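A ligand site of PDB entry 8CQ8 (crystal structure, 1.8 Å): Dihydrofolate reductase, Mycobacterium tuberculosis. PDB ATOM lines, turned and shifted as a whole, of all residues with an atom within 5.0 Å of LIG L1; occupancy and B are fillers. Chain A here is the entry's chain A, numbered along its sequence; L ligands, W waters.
The backbone NH of Arg 69 is in hydrogen-bond range of an oxygen (O15) of LIG L1, 2.7 Å away.
The backbone carbonyl oxygen of Ala 9 is in hydrogen-bond range of a nitrogen (N7) of LIG L1 (2.9 Å).
The backbone carbonyl oxygen of Ile 96 is in hydrogen-bond range of a nitrogen (N3) of LG2 L2 (3.0 Å).
N of Asp 21 sits at hydrogen-bond distance from O12 of LIG L1.
N3 of LG2 L2 lies within hydrogen-bond range of OH of Tyr 102 (3.2 Å).
The backbone NH (N) of Ala 9 sits at hydrogen-bond distance from an oxygen (O14) of LIG L1 (2.8 Å).
The guanidinium group (NH1) of Arg 47 lies within salt-bridge range of an oxygen (O8) of LIG L1 (3.5 Å).
A nitrogen (N5) of LIG L1 sits close to the backbone NH (N) of Ser 68 (3.5 Å).
N of Gly 98 lies within hydrogen-bond range of O1 of LIG L1.
O17 of LIG L1 is in hydrogen-bond range of OG of Ser 68, at 2.8 Å.
A nitrogen (N2) of LG2 L2 lies close to the backbone NH (N) of Trp 8 (3.3 Å).
An oxygen (O2) of LIG L1 sits at hydrogen-bond distance from the backbone NH (N) of Val 101 (3.4 Å).
An oxygen (O9) of LIG L1 sits at hydrogen-bond distance from the backbone NH (N) of Gln 100 (2.7 Å).
An oxygen (O1) of LIG L1 is in hydrogen-bond range of the backbone NH of Thr 48 (3.2 Å).
The guanidinium group (NH2) of Arg 46 is in salt-bridge range of an oxygen (O16) of LIG L1.
OG1 of Thr 48 lies within hydrogen-bond range of O1 of LIG L1.
The backbone NH of Arg 47 lies within hydrogen-bond range of an oxygen (O3) of LIG L1 (3.3 Å).
The backbone NH (N) of Gly 99 lies within hydrogen-bond range of an oxygen (O9) of LIG L1 (3.0 Å).
The backbone NH (N) of Arg 46 sits at hydrogen-bond distance from an oxygen (O3) of LIG L1 (3.5 Å).
The backbone carbonyl oxygen (O) of Ile 7 is in hydrogen-bond range of a nitrogen (N3) of LG2 L2 (2.6 Å).
The backbone carbonyl oxygen (O) of Asp 21 lies within hydrogen-bond range of an oxygen (O12) of LIG L1, at 3.0 Å.
N7 of LIG L1 is in hydrogen-bond range of O of Ile 16.
The backbone carbonyl oxygen (O) of Leu 67 sits at hydrogen-bond distance from the backbone NH (N) of Arg 46 (3.0 Å).
The side-chain hydroxyl (OG) of Ser 68 is in hydrogen-bond range of the backbone NH (N) of Gln 70 (3.0 Å).
The backbone carbonyl oxygen of Ile 96 sits at hydrogen-bond distance from the side-chain hydroxyl of Tyr 102.
The side-chain hydroxyl (OH) of Tyr 102 is in hydrogen-bond range of the backbone carbonyl oxygen (O) of Ile 7 (2.6 Å).
The backbone NH of Ile 16 sits at hydrogen-bond distance from the backbone carbonyl oxygen of Ala 128, at 2.8 Å.
The side-chain amide nitrogen of Gln 100 lies close to the guanidinium group of Arg 47 (3.3 Å).
The backbone carbonyl oxygen (O) of Thr 48 lies within hydrogen-bond range of the side-chain hydroxyl (OG) of Ser 51, at 2.7 Å.
OG1 of Thr 48 sits at hydrogen-bond distance from N of Gly 98, at 3.0 Å.
O of Leu 67 sits close to O4 of LIG L1 (3.5 Å).
Residues that only touch LIG L1: Gly 20, Ile 96, Gly 45, Trp 8, Gly 17, Tyr 102, Gly 82, Arg 18, Ala 128, Gln 70, Ile 22, Gly 97 and Leu 104.
Hydrophobic or aromatic side chains that line LIG L1: Trp 8, Ala 9, Ile 16, Ile 22, Leu 67, Val 101, Leu 104 and Ala 128.
Within 4 Å of LIG L1: Trp 8, Ala 9, Ile 16, Gly 17, Arg 18, Gly 20, Asp 21, Ile 22, Gly 45, Arg 46, Arg 47, Thr 48, Leu 67, Ser 68, Arg 69, Gln 70, Gly 82, Ile 96, Gly 97, Gly 98, Gly 99, Gln 100, Val 101, Tyr 102, Leu 104 and Ala 128.
The nearest printed residue that does not touch LIG L1 is Trp 24 (4.1 Å).
Water W2 bridges NH1 of Arg 69 and O15 of LIG L1.
Water W3 lies within hydrogen-bond range of an oxygen (O13) of LIG L1 and the side-chain hydroxyl (OG) of Ser 51.
Water W1 lies within hydrogen-bond range of the backbone NH (N) of Gly 20 and an oxygen (O12) of LIG L1.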
ATOM      1  N   ILE A   7     -21.950  29.330  28.942  1.00  0.00           N
ATOM      2  CA  ILE A   7     -20.650  29.967  28.814  1.00  0.00           C
ATOM      3  C   ILE A   7     -19.658  28.960  28.238  1.00  0.00           C
ATOM      4  O   ILE A   7     -19.614  27.806  28.691  1.00  0.00           O
ATOM      5  CB  ILE A   7     -20.195  30.541  30.172  1.00  0.00           C
ATOM      6  CG1 ILE A   7     -18.847  31.251  30.030  1.00  0.00           C
ATOM      7  CG2 ILE A   7     -20.204  29.465  31.267  1.00  0.00           C
ATOM      8  CD1 ILE A   7     -18.553  32.245  31.124  1.00  0.00           C
ATOM      9  N   TRP A   8     -18.881  29.371  27.228  1.00  0.00           N
ATOM     10  CA  TRP A   8     -17.883  28.499  26.601  1.00  0.00           C
ATOM     11  C   TRP A   8     -16.832  29.349  25.915  1.00  0.00           C
ATOM     12  O   TRP A   8     -17.070  30.508  25.576  1.00  0.00           O
ATOM     13  CB  TRP A   8     -18.500  27.557  25.567  1.00  0.00           C
ATOM     14  CG  TRP A   8     -18.922  28.178  24.251  1.00  0.00           C
ATOM     15  CD1 TRP A   8     -18.116  28.565  23.208  1.00  0.00           C
ATOM     16  CD2 TRP A   8     -20.269  28.408  23.815  1.00  0.00           C
ATOM     17  NE1 TRP A   8     -18.878  29.048  22.175  1.00  0.00           N
ATOM     18  CE2 TRP A   8     -20.197  28.962  22.517  1.00  0.00           C
ATOM     19  CE3 TRP A   8     -21.521  28.214  24.392  1.00  0.00           C
ATOM     20  CZ2 TRP A   8     -21.337  29.330  21.800  1.00  0.00           C
ATOM     21  CZ3 TRP A   8     -22.640  28.569  23.691  1.00  0.00           C
ATOM     22  CH2 TRP A   8     -22.548  29.123  22.404  1.00  0.00           C
ATOM     23  N   ALA A   9     -15.670  28.729  25.676  1.00  0.00           N
ATOM     24  CA  ALA A   9     -14.605  29.312  24.865  1.00  0.00           C
ATOM     25  C   ALA A   9     -14.435  28.445  23.634  1.00  0.00           C
ATOM     26  O   ALA A   9     -14.402  27.228  23.733  1.00  0.00           O
ATOM     27  CB  ALA A   9     -13.298  29.399  25.632  1.00  0.00           C
ATOM     28  N   ILE A  16     -14.486  23.401  20.764  1.00  0.00           N
ATOM     29  CA  ILE A  16     -14.388  23.758  22.165  1.00  0.00           C
ATOM     30  C   ILE A  16     -13.573  22.754  22.986  1.00  0.00           C
ATOM     31  O   ILE A  16     -12.974  23.151  24.006  1.00  0.00           O
ATOM     32  CB  ILE A  16     -15.783  23.935  22.784  1.00  0.00           C
ATOM     33  CG1 ILE A  16     -16.533  22.613  22.819  1.00  0.00           C
ATOM     34  CG2 ILE A  16     -16.575  24.976  21.968  1.00  0.00           C
ATOM     35  CD1 ILE A  16     -17.580  22.474  23.928  1.00  0.00           C
ATOM     36  N   GLY A  17     -13.524  21.480  22.605  1.00  0.00           N
ATOM     37  CA  GLY A  17     -12.709  20.485  23.277  1.00  0.00           C
ATOM     38  C   GLY A  17     -12.167  19.468  22.291  1.00  0.00           C
ATOM     39  O   GLY A  17     -12.713  19.278  21.207  1.00  0.00           O
ATOM     40  N   ARG A  18     -11.085  18.806  22.699  1.00  0.00           N
ATOM     41  CA  ARG A  18     -10.408  17.822  21.867  1.00  0.00           C
ATOM     42  C   ARG A  18      -9.600  16.920  22.785  1.00  0.00           C
ATOM     43  O   ARG A  18      -8.841  17.401  23.620  1.00  0.00           O
ATOM     44  CB  ARG A  18      -9.506  18.524  20.847  1.00  0.00           C
ATOM     45  CG  ARG A  18      -8.649  17.614  20.022  1.00  0.00           C
ATOM     46  CD  ARG A  18      -7.878  18.368  18.962  1.00  0.00           C
ATOM     47  NE  ARG A  18      -8.753  18.862  17.892  1.00  0.00           N
ATOM     48  CZ  ARG A  18      -8.314  19.578  16.864  1.00  0.00           C
ATOM     49  NH1 ARG A  18      -7.013  19.852  16.777  1.00  0.00           N
ATOM     50  NH2 ARG A  18      -9.158  19.982  15.919  1.00  0.00           N
ATOM     51  N   GLY A  19      -9.775  15.606  22.629  1.00  0.00           N
ATOM     52  CA  GLY A  19      -9.124  14.675  23.527  1.00  0.00           C
ATOM     53  C   GLY A  19      -9.535  14.857  24.970  1.00  0.00           C
ATOM     54  O   GLY A  19      -8.710  14.657  25.873  1.00  0.00           O
ATOM     55  N   GLY A  20     -10.776  15.265  25.217  1.00  0.00           N
ATOM     56  CA  GLY A  20     -11.225  15.404  26.588  1.00  0.00           C
ATOM     57  C   GLY A  20     -10.682  16.608  27.333  1.00  0.00           C
ATOM     58  O   GLY A  20     -10.692  16.603  28.582  1.00  0.00           O
ATOM     59  N   ASP A  21     -10.240  17.634  26.622  1.00  0.00           N
ATOM     60  CA  ASP A  21      -9.702  18.791  27.293  1.00  0.00           C
ATOM     61  C   ASP A  21      -9.654  19.903  26.266  1.00  0.00           C
ATOM     62  O   ASP A  21     -10.382  19.869  25.262  1.00  0.00           O
ATOM     63  CB  ASP A  21      -8.396  18.354  27.902  1.00  0.00           C
ATOM     64  CG  ASP A  21      -7.854  19.362  28.791  1.00  0.00           C
ATOM     65  OD1 ASP A  21      -8.425  20.453  28.994  1.00  0.00           O
ATOM     66  OD2 ASP A  21      -6.858  19.043  29.391  1.00  0.00           O
ATOM     67  N   ILE A  22      -8.768  20.891  26.435  1.00  0.00           N
ATOM     68  CA  ILE A  22      -8.871  22.141  25.676  1.00  0.00           C
ATOM     69  C   ILE A  22      -7.502  22.468  25.088  1.00  0.00           C
ATOM     70  O   ILE A  22      -6.529  22.594  25.834  1.00  0.00           O
ATOM     71  CB  ILE A  22      -9.369  23.271  26.579  1.00  0.00           C
ATOM     72  CG1 ILE A  22     -10.700  22.849  27.202  1.00  0.00           C
ATOM     73  CG2 ILE A  22      -9.536  24.542  25.787  1.00  0.00           C
ATOM     74  CD1 ILE A  22     -11.181  23.735  28.294  1.00  0.00           C
ATOM     75  N   TRP A  24      -5.885  25.009  24.419  1.00  0.00           N
ATOM     76  CA  TRP A  24      -5.430  26.349  24.723  1.00  0.00           C
ATOM     77  C   TRP A  24      -5.667  26.615  26.199  1.00  0.00           C
ATOM     78  O   TRP A  24      -6.384  25.879  26.885  1.00  0.00           O
ATOM     79  CB  TRP A  24      -6.151  27.401  23.867  1.00  0.00           C
ATOM     80  CG  TRP A  24      -7.608  27.426  24.106  1.00  0.00           C
ATOM     81  CD1 TRP A  24      -8.257  27.943  25.185  1.00  0.00           C
ATOM     82  CD2 TRP A  24      -8.618  26.997  23.189  1.00  0.00           C
ATOM     83  NE1 TRP A  24      -9.610  27.806  25.028  1.00  0.00           N
ATOM     84  CE2 TRP A  24      -9.860  27.233  23.808  1.00  0.00           C
ATOM     85  CE3 TRP A  24      -8.595  26.405  21.935  1.00  0.00           C
ATOM     86  CZ2 TRP A  24     -11.060  26.911  23.210  1.00  0.00           C
ATOM     87  CZ3 TRP A  24      -9.785  26.085  21.338  1.00  0.00           C
ATOM     88  CH2 TRP A  24     -11.002  26.341  21.977  1.00  0.00           C
ATOM     89  N   GLY A  45     -21.365  18.390  31.941  1.00  0.00           N
ATOM     90  CA  GLY A  45     -21.436  16.974  31.643  1.00  0.00           C
ATOM     91  C   GLY A  45     -20.392  16.173  32.405  1.00  0.00           C
ATOM     92  O   GLY A  45     -19.402  16.701  32.898  1.00  0.00           O
ATOM     93  N   ARG A  46     -20.636  14.861  32.491  1.00  0.00           N
ATOM     94  CA  ARG A  46     -19.736  14.009  33.266  1.00  0.00           C
ATOM     95  C   ARG A  46     -18.326  13.996  32.662  1.00  0.00           C
ATOM     96  O   ARG A  46     -17.335  13.942  33.396  1.00  0.00           O
ATOM     97  CB  ARG A  46     -20.295  12.588  33.353  1.00  0.00           C
ATOM     98  CG  ARG A  46     -19.672  11.723  34.442  1.00  0.00           C
ATOM     99  CD  ARG A  46     -18.561  10.865  33.896  1.00  0.00           C
ATOM    100  NE  ARG A  46     -19.060  10.140  32.736  1.00  0.00           N
ATOM    101  CZ  ARG A  46     -18.296   9.677  31.754  1.00  0.00           C
ATOM    102  NH1 ARG A  46     -16.976   9.863  31.803  1.00  0.00           N
ATOM    103  NH2 ARG A  46     -18.844   9.038  30.729  1.00  0.00           N
ATOM    104  N   ARG A  47     -18.232  14.067  31.332  1.00  0.00           N
ATOM    105  CA  ARG A  47     -16.911  14.144  30.703  1.00  0.00           C
ATOM    106  C   ARG A  47     -16.170  15.383  31.167  1.00  0.00           C
ATOM    107  O   ARG A  47     -14.985  15.332  31.486  1.00  0.00           O
ATOM    108  CB  ARG A  47     -17.000  14.132  29.178  1.00  0.00           C
ATOM    109  CG  ARG A  47     -17.635  12.881  28.566  1.00  0.00           C
ATOM    110  CD  ARG A  47     -17.206  12.623  27.101  1.00  0.00           C
ATOM    111  NE  ARG A  47     -18.001  11.531  26.550  1.00  0.00           N
ATOM    112  CZ  ARG A  47     -18.363  11.412  25.276  1.00  0.00           C
ATOM    113  NH1 ARG A  47     -17.962  12.315  24.361  1.00  0.00           N
ATOM    114  NH2 ARG A  47     -19.114  10.387  24.904  1.00  0.00           N
ATOM    115  N   THR A  48     -16.885  16.518  31.238  1.00  0.00           N
ATOM    116  CA  THR A  48     -16.278  17.762  31.694  1.00  0.00           C
ATOM    117  C   THR A  48     -15.845  17.671  33.160  1.00  0.00           C
ATOM    118  O   THR A  48     -14.741  18.094  33.520  1.00  0.00           O
ATOM    119  CB  THR A  48     -17.256  18.900  31.455  1.00  0.00           C
ATOM    120  OG1 THR A  48     -17.476  19.030  30.046  1.00  0.00           O
ATOM    121  CG2 THR A  48     -16.672  20.195  31.934  1.00  0.00           C
ATOM    122  N   SER A  51     -12.721  16.013  33.297  1.00  0.00           N
ATOM    123  CA  SER A  51     -11.596  16.824  32.821  1.00  0.00           C
ATOM    124  C   SER A  51     -11.015  17.725  33.904  1.00  0.00           C
ATOM    125  O   SER A  51      -9.996  18.379  33.656  1.00  0.00           O
ATOM    126  CB  SER A  51     -12.025  17.684  31.618  1.00  0.00           C
ATOM    127  OG  SER A  51     -12.647  18.898  32.026  1.00  0.00           O
ATOM    128  N   LEU A  67     -24.274  16.223  35.008  1.00  0.00           N
ATOM    129  CA  LEU A  67     -25.176  15.304  34.303  1.00  0.00           C
ATOM    130  C   LEU A  67     -24.477  14.008  33.924  1.00  0.00           C
ATOM    131  O   LEU A  67     -23.434  14.011  33.258  1.00  0.00           O
ATOM    132  CB  LEU A  67     -25.743  15.916  33.029  1.00  0.00           C
ATOM    133  CG  LEU A  67     -26.778  17.010  32.990  1.00  0.00           C
ATOM    134  CD1 LEU A  67     -26.935  17.393  31.546  1.00  0.00           C
ATOM    135  CD2 LEU A  67     -28.061  16.368  33.452  1.00  0.00           C
ATOM    136  N   SER A  68     -25.101  12.887  34.314  1.00  0.00           N
ATOM    137  CA  SER A  68     -24.613  11.540  34.037  1.00  0.00           C
ATOM    138  C   SER A  68     -25.816  10.627  33.904  1.00  0.00           C
ATOM    139  O   SER A  68     -26.818  10.812  34.597  1.00  0.00           O
ATOM    140  CB  SER A  68     -23.695  11.016  35.148  1.00  0.00           C
ATOM    141  OG  SER A  68     -23.382   9.647  34.928  1.00  0.00           O
ATOM    142  N   ARG A  69     -25.707   9.630  33.043  1.00  0.00           N
ATOM    143  CA  ARG A  69     -26.733   8.591  32.963  1.00  0.00           C
ATOM    144  C   ARG A  69     -26.459   7.439  33.902  1.00  0.00           C
ATOM    145  O   ARG A  69     -27.355   6.611  34.106  1.00  0.00           O
ATOM    146  CB  ARG A  69     -26.861   8.101  31.516  1.00  0.00           C
ATOM    147  CG  ARG A  69     -27.263   9.193  30.542  1.00  0.00           C
ATOM    148  CD  ARG A  69     -28.316   8.739  29.581  1.00  0.00           C
ATOM    149  NE  ARG A  69     -28.470   9.710  28.508  1.00  0.00           N
ATOM    150  CZ  ARG A  69     -27.686   9.770  27.435  1.00  0.00           C
ATOM    151  NH1 ARG A  69     -26.659   8.924  27.308  1.00  0.00           N
ATOM    152  NH2 ARG A  69     -27.899  10.683  26.490  1.00  0.00           N
ATOM    153  N   GLN A  70     -25.257   7.363  34.493  1.00  0.00           N
ATOM    154  CA  GLN A  70     -24.947   6.429  35.569  1.00  0.00           C
ATOM    155  C   GLN A  70     -25.654   6.852  36.858  1.00  0.00           C
ATOM    156  O   GLN A  70     -25.215   7.800  37.517  1.00  0.00           O
ATOM    157  CB  GLN A  70     -23.440   6.380  35.829  1.00  0.00           C
ATOM    158  CG  GLN A  70     -22.524   5.878  34.710  1.00  0.00           C
ATOM    159  CD  GLN A  70     -21.043   5.956  35.101  1.00  0.00           C
ATOM    160  OE1 GLN A  70     -20.623   5.436  36.156  1.00  0.00           O
ATOM    161  NE2 GLN A  70     -20.240   6.626  34.255  1.00  0.00           N
ATOM    162  N   GLY A  82     -29.566  13.121  36.679  1.00  0.00           N
ATOM    163  CA  GLY A  82     -29.716  12.363  35.455  1.00  0.00           C
ATOM    164  C   GLY A  82     -30.609  13.065  34.463  1.00  0.00           C
ATOM    165  O   GLY A  82     -30.814  12.581  33.346  1.00  0.00           O
ATOM    166  N   ILE A  96     -21.718  24.921  31.776  1.00  0.00           N
ATOM    167  CA  ILE A  96     -20.303  25.195  31.545  1.00  0.00           C
ATOM    168  C   ILE A  96     -19.628  24.144  30.662  1.00  0.00           C
ATOM    169  O   ILE A  96     -18.391  24.150  30.538  1.00  0.00           O
ATOM    170  CB  ILE A  96     -19.551  25.388  32.867  1.00  0.00           C
ATOM    171  CG1 ILE A  96     -19.482  24.128  33.709  1.00  0.00           C
ATOM    172  CG2 ILE A  96     -20.178  26.485  33.671  1.00  0.00           C
ATOM    173  CD1 ILE A  96     -18.476  24.254  34.835  1.00  0.00           C
ATOM    174  N   GLY A  97     -20.393  23.284  30.003  1.00  0.00           N
ATOM    175  CA  GLY A  97     -19.868  22.350  29.020  1.00  0.00           C
ATOM    176  C   GLY A  97     -20.144  20.900  29.384  1.00  0.00           C
ATOM    177  O   GLY A  97     -20.689  20.581  30.441  1.00  0.00           O
ATOM    178  N   GLY A  98     -19.758  20.020  28.459  1.00  0.00           N
ATOM    179  CA  GLY A  98     -19.179  20.400  27.177  1.00  0.00           C
ATOM    180  C   GLY A  98     -20.188  20.282  26.055  1.00  0.00           C
ATOM    181  O   GLY A  98     -21.378  20.452  26.287  1.00  0.00           O
ATOM    182  N   GLY A  99     -19.717  19.931  24.854  1.00  0.00           N
ATOM    183  CA  GLY A  99     -20.534  20.053  23.646  1.00  0.00           C
ATOM    184  C   GLY A  99     -21.864  19.329  23.727  1.00  0.00           C
ATOM    185  O   GLY A  99     -22.871  19.824  23.203  1.00  0.00           O
ATOM    186  N   GLN A 100     -21.887  18.144  24.342  1.00  0.00           N
ATOM    187  CA  GLN A 100     -23.151  17.433  24.482  1.00  0.00           C
ATOM    188  C   GLN A 100     -24.118  18.218  25.353  1.00  0.00           C
ATOM    189  O   GLN A 100     -25.263  18.443  24.966  1.00  0.00           O
ATOM    190  CB  GLN A 100     -22.937  16.019  25.038  1.00  0.00           C
ATOM    191  CG  GLN A 100     -22.134  15.109  24.105  1.00  0.00           C
ATOM    192  CD  GLN A 100     -22.096  13.642  24.555  1.00  0.00           C
ATOM    193  OE1 GLN A 100     -22.870  13.213  25.428  1.00  0.00           O
ATOM    194  NE2 GLN A 100     -21.201  12.864  23.937  1.00  0.00           N
ATOM    195  N   VAL A 101     -23.653  18.667  26.516  1.00  0.00           N
ATOM    196  CA  VAL A 101     -24.551  19.350  27.430  1.00  0.00           C
ATOM    197  C   VAL A 101     -24.957  20.707  26.874  1.00  0.00           C
ATOM    198  O   VAL A 101     -26.099  21.142  27.087  1.00  0.00           O
ATOM    199  CB  VAL A 101     -23.929  19.457  28.826  1.00  0.00           C
ATOM    200  CG1 VAL A 101     -24.868  20.184  29.770  1.00  0.00           C
ATOM    201  CG2 VAL A 101     -23.669  18.078  29.353  1.00  0.00           C
ATOM    202  N   TYR A 102     -24.079  21.380  26.114  1.00  0.00           N
ATOM    203  CA  TYR A 102     -24.492  22.643  25.486  1.00  0.00           C
ATOM    204  C   TYR A 102     -25.691  22.421  24.604  1.00  0.00           C
ATOM    205  O   TYR A 102     -26.656  23.196  24.645  1.00  0.00           O
ATOM    206  CB  TYR A 102     -23.376  23.282  24.654  1.00  0.00           C
ATOM    207  CG  TYR A 102     -22.239  23.884  25.448  1.00  0.00           C
ATOM    208  CD1 TYR A 102     -20.943  23.891  24.942  1.00  0.00           C
ATOM    209  CD2 TYR A 102     -22.450  24.389  26.721  1.00  0.00           C
ATOM    210  CE1 TYR A 102     -19.882  24.428  25.688  1.00  0.00           C
ATOM    211  CE2 TYR A 102     -21.406  24.913  27.462  1.00  0.00           C
ATOM    212  CZ  TYR A 102     -20.132  24.933  26.940  1.00  0.00           C
ATOM    213  OH  TYR A 102     -19.095  25.438  27.695  1.00  0.00           O
ATOM    214  N   LEU A 104     -27.824  20.028  24.768  1.00  0.00           N
ATOM    215  CA  LEU A 104     -28.975  19.656  25.584  1.00  0.00           C
ATOM    216  C   LEU A 104     -29.615  20.861  26.260  1.00  0.00           C
ATOM    217  O   LEU A 104     -30.822  20.852  26.535  1.00  0.00           O
ATOM    218  CB  LEU A 104     -28.548  18.624  26.615  1.00  0.00           C
ATOM    219  CG  LEU A 104     -29.623  18.049  27.528  1.00  0.00           C
ATOM    220  CD1 LEU A 104     -30.608  17.202  26.768  1.00  0.00           C
ATOM    221  CD2 LEU A 104     -28.958  17.229  28.615  1.00  0.00           C
ATOM    222  N   ALA A 128     -15.157  18.198  20.479  1.00  0.00           N
ATOM    223  CA  ALA A 128     -16.386  18.792  21.001  1.00  0.00           C
ATOM    224  C   ALA A 128     -16.609  20.177  20.378  1.00  0.00           C
ATOM    225  O   ALA A 128     -15.651  20.893  20.081  1.00  0.00           O
ATOM    226  CB  ALA A 128     -16.370  18.908  22.529  1.00  0.00           C
HETATM  227  P1  LIG L   1     -19.798  16.305  28.027  1.00  0.00           P
HETATM  228  O1  LIG L   1     -18.905  17.187  28.835  1.00  0.00           O
HETATM  229  O2  LIG L   1     -20.902  16.844  27.165  1.00  0.00           O
HETATM  230  O3  LIG L   1     -20.328  15.196  29.062  1.00  0.00           O
HETATM  231  C1  LIG L   1     -21.028  14.294  28.329  1.00  0.00           C
HETATM  232  C2  LIG L   1     -21.619  13.424  29.370  1.00  0.00           C
HETATM  233  O4  LIG L   1     -22.760  14.052  29.861  1.00  0.00           O
HETATM  234  C3  LIG L   1     -22.046  12.088  28.817  1.00  0.00           C
HETATM  235  O5  LIG L   1     -20.959  11.203  28.814  1.00  0.00           O
HETATM  236  C4  LIG L   1     -23.061  11.687  29.955  1.00  0.00           C
HETATM  237  O6  LIG L   1     -22.490  11.350  31.085  1.00  0.00           O
HETATM  238  C5  LIG L   1     -23.695  13.050  30.242  1.00  0.00           C
HETATM  239  N1  LIG L   1     -24.859  13.250  29.486  1.00  0.00           N
HETATM  240  C6  LIG L   1     -24.973  13.719  28.176  1.00  0.00           C
HETATM  241  N2  LIG L   1     -26.250  13.801  27.763  1.00  0.00           N
HETATM  242  C7  LIG L   1     -26.983  13.337  28.870  1.00  0.00           C
HETATM  243  C8  LIG L   1     -28.340  13.188  29.077  1.00  0.00           C
HETATM  244  N3  LIG L   1     -29.214  13.516  28.056  1.00  0.00           N
HETATM  245  N4  LIG L   1     -28.843  12.721  30.266  1.00  0.00           N
HETATM  246  C9  LIG L   1     -27.899  12.426  31.224  1.00  0.00           C
HETATM  247  N5  LIG L   1     -26.564  12.522  31.180  1.00  0.00           N
HETATM  248  C10 LIG L   1     -26.132  12.998  29.952  1.00  0.00           C
HETATM  249  O7  LIG L   1     -18.728  15.564  27.031  1.00  0.00           O
HETATM  250  P2  LIG L   1     -18.357  16.403  25.731  1.00  0.00           P
HETATM  251  O8  LIG L   1     -17.236  15.683  25.080  1.00  0.00           O
HETATM  252  O9  LIG L   1     -19.493  16.899  24.872  1.00  0.00           O
HETATM  253  O10 LIG L   1     -17.516  17.850  26.183  1.00  0.00           O
HETATM  254  C11 LIG L   1     -16.307  17.493  26.785  1.00  0.00           C
HETATM  255  C12 LIG L   1     -15.201  18.245  26.045  1.00  0.00           C
HETATM  256  O11 LIG L   1     -15.494  19.663  25.980  1.00  0.00           O
HETATM  257  C13 LIG L   1     -13.820  18.135  26.792  1.00  0.00           C
HETATM  258  O12 LIG L   1     -12.816  18.279  25.828  1.00  0.00           O
HETATM  259  C14 LIG L   1     -13.845  19.375  27.627  1.00  0.00           C
HETATM  260  O13 LIG L   1     -12.579  19.813  27.968  1.00  0.00           O
HETATM  261  C15 LIG L   1     -14.401  20.348  26.582  1.00  0.00           C
HETATM  262  N6  LIG L   1     -14.897  21.542  27.262  1.00  0.00           N
HETATM  263  C16 LIG L   1     -14.638  22.786  26.745  1.00  0.00           C
HETATM  264  C17 LIG L   1     -15.143  23.912  27.342  1.00  0.00           C
HETATM  265  C18 LIG L   1     -14.819  25.223  26.733  1.00  0.00           C
HETATM  266  O14 LIG L   1     -15.384  26.298  27.027  1.00  0.00           O
HETATM  267  N7  LIG L   1     -13.791  25.245  25.781  1.00  0.00           N
HETATM  268  C19 LIG L   1     -15.997  23.842  28.554  1.00  0.00           C
HETATM  269  C20 LIG L   1     -16.133  22.454  29.062  1.00  0.00           C
HETATM  270  C21 LIG L   1     -15.612  21.407  28.444  1.00  0.00           C
HETATM  271  P3  LIG L   1     -22.408   9.568  31.281  1.00  0.00           P
HETATM  272  O15 LIG L   1     -23.874   9.332  31.137  1.00  0.00           O
HETATM  273  O16 LIG L   1     -21.486   9.205  30.101  1.00  0.00           O
HETATM  274  O17 LIG L   1     -21.801   9.507  32.670  1.00  0.00           O
HETATM  275  C1  LG2 L   2     -14.185  22.496  33.063  1.00  0.00           C
HETATM  276  C2  LG2 L   2     -12.703  27.480  31.176  1.00  0.00           C
HETATM  277  C3  LG2 L   2     -10.856  25.927  31.519  1.00  0.00           C
HETATM  278  C4  LG2 L   2      -8.916  26.302  33.031  1.00  0.00           C
HETATM  279  C5  LG2 L   2     -10.848  27.958  32.712  1.00  0.00           C
HETATM  280  C6  LG2 L   2     -12.056  28.319  32.101  1.00  0.00           C
HETATM  281  C7  LG2 L   2     -15.170  29.498  29.324  1.00  0.00           C
HETATM  282  C8  LG2 L   2     -16.346  27.615  30.061  1.00  0.00           C
HETATM  283  C9  LG2 L   2     -15.172  27.123  30.670  1.00  0.00           C
HETATM  284  C10 LG2 L   2     -15.201  25.900  31.345  1.00  0.00           C
HETATM  285  C11 LG2 L   2     -15.096  24.926  31.983  1.00  0.00           C
HETATM  286  C12 LG2 L   2     -14.855  23.820  32.823  1.00  0.00           C
HETATM  287  C13 LG2 L   2     -14.921  23.259  34.193  1.00  0.00           C
HETATM  288  C14 LG2 L   2     -14.020  27.881  30.541  1.00  0.00           C
HETATM  289  C15 LG2 L   2     -12.052  26.281  30.905  1.00  0.00           C
HETATM  290  C16 LG2 L   2     -10.215  26.751  32.426  1.00  0.00           C
HETATM  291  C17 LG2 L   2      -7.023  26.705  34.402  1.00  0.00           C
HETATM  292  N1  LG2 L   2     -15.219  30.709  28.635  1.00  0.00           N
HETATM  293  N2  LG2 L   2     -16.373  28.817  29.378  1.00  0.00           N
HETATM  294  N3  LG2 L   2     -17.535  26.971  30.087  1.00  0.00           N
HETATM  295  N4  LG2 L   2     -13.988  29.075  29.909  1.00  0.00           N
HETATM  296  O1  LG2 L   2      -8.253  27.152  33.840  1.00  0.00           O
HETATM  297  O2  LG2 L   2      -8.407  25.213  32.841  1.00  0.00           O
HETATM  298  O   HOH W   1     -13.120  16.080  23.850  1.00  0.00           O
HETATM  299  O   HOH W   2     -24.778   8.339  28.868  1.00  0.00           O
HETATM  300  O   HOH W   3     -12.133  20.956  30.330  1.00  0.00           O
HETATM  301  O   HOH W   4     -19.305  16.294  21.980  1.00  0.00           O
